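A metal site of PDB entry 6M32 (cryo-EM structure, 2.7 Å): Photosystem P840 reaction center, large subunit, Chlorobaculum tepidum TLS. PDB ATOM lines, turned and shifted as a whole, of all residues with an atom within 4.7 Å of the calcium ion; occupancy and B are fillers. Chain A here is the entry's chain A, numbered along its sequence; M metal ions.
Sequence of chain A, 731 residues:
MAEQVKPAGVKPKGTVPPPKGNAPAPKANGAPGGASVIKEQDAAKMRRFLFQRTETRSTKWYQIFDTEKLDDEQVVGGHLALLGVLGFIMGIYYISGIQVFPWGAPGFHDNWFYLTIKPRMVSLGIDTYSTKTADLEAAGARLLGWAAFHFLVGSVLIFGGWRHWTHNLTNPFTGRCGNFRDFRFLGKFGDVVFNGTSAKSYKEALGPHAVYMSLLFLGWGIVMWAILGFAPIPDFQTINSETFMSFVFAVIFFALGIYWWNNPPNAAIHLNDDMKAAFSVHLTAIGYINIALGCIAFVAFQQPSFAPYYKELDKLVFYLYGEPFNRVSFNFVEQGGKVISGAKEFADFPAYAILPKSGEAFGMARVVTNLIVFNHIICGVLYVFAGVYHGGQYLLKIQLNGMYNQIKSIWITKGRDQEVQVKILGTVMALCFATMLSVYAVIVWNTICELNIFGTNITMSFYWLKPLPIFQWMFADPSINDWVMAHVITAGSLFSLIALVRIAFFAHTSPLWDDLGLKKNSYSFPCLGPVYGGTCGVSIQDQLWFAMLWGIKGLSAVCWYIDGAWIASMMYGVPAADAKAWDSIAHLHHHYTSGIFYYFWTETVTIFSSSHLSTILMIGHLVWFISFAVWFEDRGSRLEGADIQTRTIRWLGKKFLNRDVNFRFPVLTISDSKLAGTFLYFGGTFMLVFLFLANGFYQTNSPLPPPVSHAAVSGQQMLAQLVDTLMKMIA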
ATOM      1  N   ASP A 563      22.560 -28.683 -22.016  1.00  0.00           N
ATOM      2  CA  ASP A 563      23.531 -28.691 -23.098  1.00  0.00           C
ATOM      3  C   ASP A 563      22.975 -29.276 -24.392  1.00  0.00           C
ATOM      4  O   ASP A 563      23.718 -29.395 -25.365  1.00  0.00           O
ATOM      5  CB  ASP A 563      24.782 -29.466 -22.675  1.00  0.00           C
ATOM      6  CG  ASP A 563      26.050 -28.896 -23.281  1.00  0.00           C
ATOM      7  OD1 ASP A 563      26.039 -27.700 -23.656  1.00  0.00           O
ATOM      8  OD2 ASP A 563      27.059 -29.617 -23.371  1.00  0.00           O
ATOM      9  N   GLU A 603      31.811 -34.125 -28.343  1.00  0.00           N
ATOM     10  CA  GLU A 603      32.136 -33.216 -27.260  1.00  0.00           C
ATOM     11  C   GLU A 603      33.594 -33.363 -26.862  1.00  0.00           C
ATOM     12  O   GLU A 603      34.283 -32.369 -26.653  1.00  0.00           O
ATOM     13  CB  GLU A 603      31.229 -33.473 -26.054  1.00  0.00           C
ATOM     14  CG  GLU A 603      29.810 -32.955 -26.213  1.00  0.00           C
ATOM     15  CD  GLU A 603      29.177 -32.581 -24.888  1.00  0.00           C
ATOM     16  OE1 GLU A 603      28.539 -33.458 -24.261  1.00  0.00           O
ATOM     17  OE2 GLU A 603      29.301 -31.412 -24.482  1.00  0.00           O
ATOM     18  N   PHE A 692      31.866 -30.721 -19.769  1.00  0.00           N
ATOM     19  CA  PHE A 692      30.706 -30.732 -20.648  1.00  0.00           C
ATOM     20  C   PHE A 692      30.167 -29.329 -20.878  1.00  0.00           C
ATOM     21  O   PHE A 692      29.782 -28.988 -22.004  1.00  0.00           O
ATOM     22  CB  PHE A 692      29.609 -31.627 -20.067  1.00  0.00           C
ATOM     23  CG  PHE A 692      29.842 -33.080 -20.282  1.00  0.00           C
ATOM     24  CD1 PHE A 692      30.686 -33.521 -21.289  1.00  0.00           C
ATOM     25  CD2 PHE A 692      29.238 -34.024 -19.476  1.00  0.00           C
ATOM     26  CE1 PHE A 692      30.895 -34.866 -21.496  1.00  0.00           C
ATOM     27  CE2 PHE A 692      29.444 -35.372 -19.670  1.00  0.00           C
ATOM     28  CZ  PHE A 692      30.279 -35.794 -20.682  1.00  0.00           C
ATOM     29  N   LEU A 693      30.136 -28.502 -19.837  1.00  0.00           N
ATOM     30  CA  LEU A 693      29.609 -27.149 -19.956  1.00  0.00           C
ATOM     31  C   LEU A 693      30.640 -26.193 -20.540  1.00  0.00           C
ATOM     32  O   LEU A 693      30.334 -25.440 -21.468  1.00  0.00           O
ATOM     33  CB  LEU A 693      29.156 -26.653 -18.586  1.00  0.00           C
ATOM     34  CG  LEU A 693      28.033 -27.470 -17.951  1.00  0.00           C
ATOM     35  CD1 LEU A 693      27.805 -27.039 -16.518  1.00  0.00           C
ATOM     36  CD2 LEU A 693      26.764 -27.343 -18.760  1.00  0.00           C
ATOM     37  N   ASN A 695      33.097 -26.259 -22.643  1.00  0.00           N
ATOM     38  CA  ASN A 695      33.794 -26.646 -23.859  1.00  0.00           C
ATOM     39  C   ASN A 695      33.067 -26.203 -25.112  1.00  0.00           C
ATOM     40  O   ASN A 695      33.518 -26.531 -26.220  1.00  0.00           O
ATOM     41  CB  ASN A 695      34.035 -28.155 -23.906  1.00  0.00           C
ATOM     42  CG  ASN A 695      32.808 -28.932 -24.332  1.00  0.00           C
ATOM     43  OD1 ASN A 695      31.678 -28.560 -24.037  1.00  0.00           O
ATOM     44  ND2 ASN A 695      33.036 -30.037 -25.034  1.00  0.00           N
ATOM     45  N   GLY A 696      31.964 -25.480 -24.992  1.00  0.00           N
ATOM     46  CA  GLY A 696      31.148 -25.086 -26.121  1.00  0.00           C
ATOM     47  C   GLY A 696      29.723 -25.605 -25.995  1.00  0.00           C
ATOM     48  O   GLY A 696      29.414 -26.474 -25.199  1.00  0.00           O
ATOM     49  N   PHE A 697      28.858 -25.025 -26.824  1.00  0.00           N
ATOM     50  CA  PHE A 697      27.460 -25.429 -26.853  1.00  0.00           C
ATOM     51  C   PHE A 697      27.205 -26.469 -27.938  1.00  0.00           C
ATOM     52  O   PHE A 697      26.790 -27.589 -27.648  1.00  0.00           O
ATOM     53  CB  PHE A 697      26.565 -24.203 -27.048  1.00  0.00           C
ATOM     54  CG  PHE A 697      25.111 -24.470 -26.818  1.00  0.00           C
ATOM     55  CD1 PHE A 697      24.708 -25.393 -25.870  1.00  0.00           C
ATOM     56  CD2 PHE A 697      24.152 -23.819 -27.551  1.00  0.00           C
ATOM     57  CE1 PHE A 697      23.389 -25.657 -25.659  1.00  0.00           C
ATOM     58  CE2 PHE A 697      22.816 -24.067 -27.349  1.00  0.00           C
ATOM     59  CZ  PHE A 697      22.437 -24.993 -26.397  1.00  0.00           C
HETATM   60 CA    CA M   1      29.198 -28.707 -24.316  1.00  0.00          CA
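Five residues have an atom within 4 Å of the calcium ion: Asp 563, Glu 603, Phe 692, Asn 695 and Gly 696.
The nearest printed residue that does not touch the calcium ion is Phe 697 (4.3 Å).
The backbone carbonyl oxygen (O) of Phe 692 binds the calcium ion (2.4 Å).
O of Gly 696 is bound to the calcium ion.
OD1 of Asn 695 is bound to the calcium ion, at 2.5 Å.
The calcium ion is bound by the side-chain carboxylate (OD2) of Asp 563, at 2.5 Å.
The calcium ion is bound by OE2 of Glu 603, at 2.7 Å.
The calcium ion has five donor atoms within binding distance.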
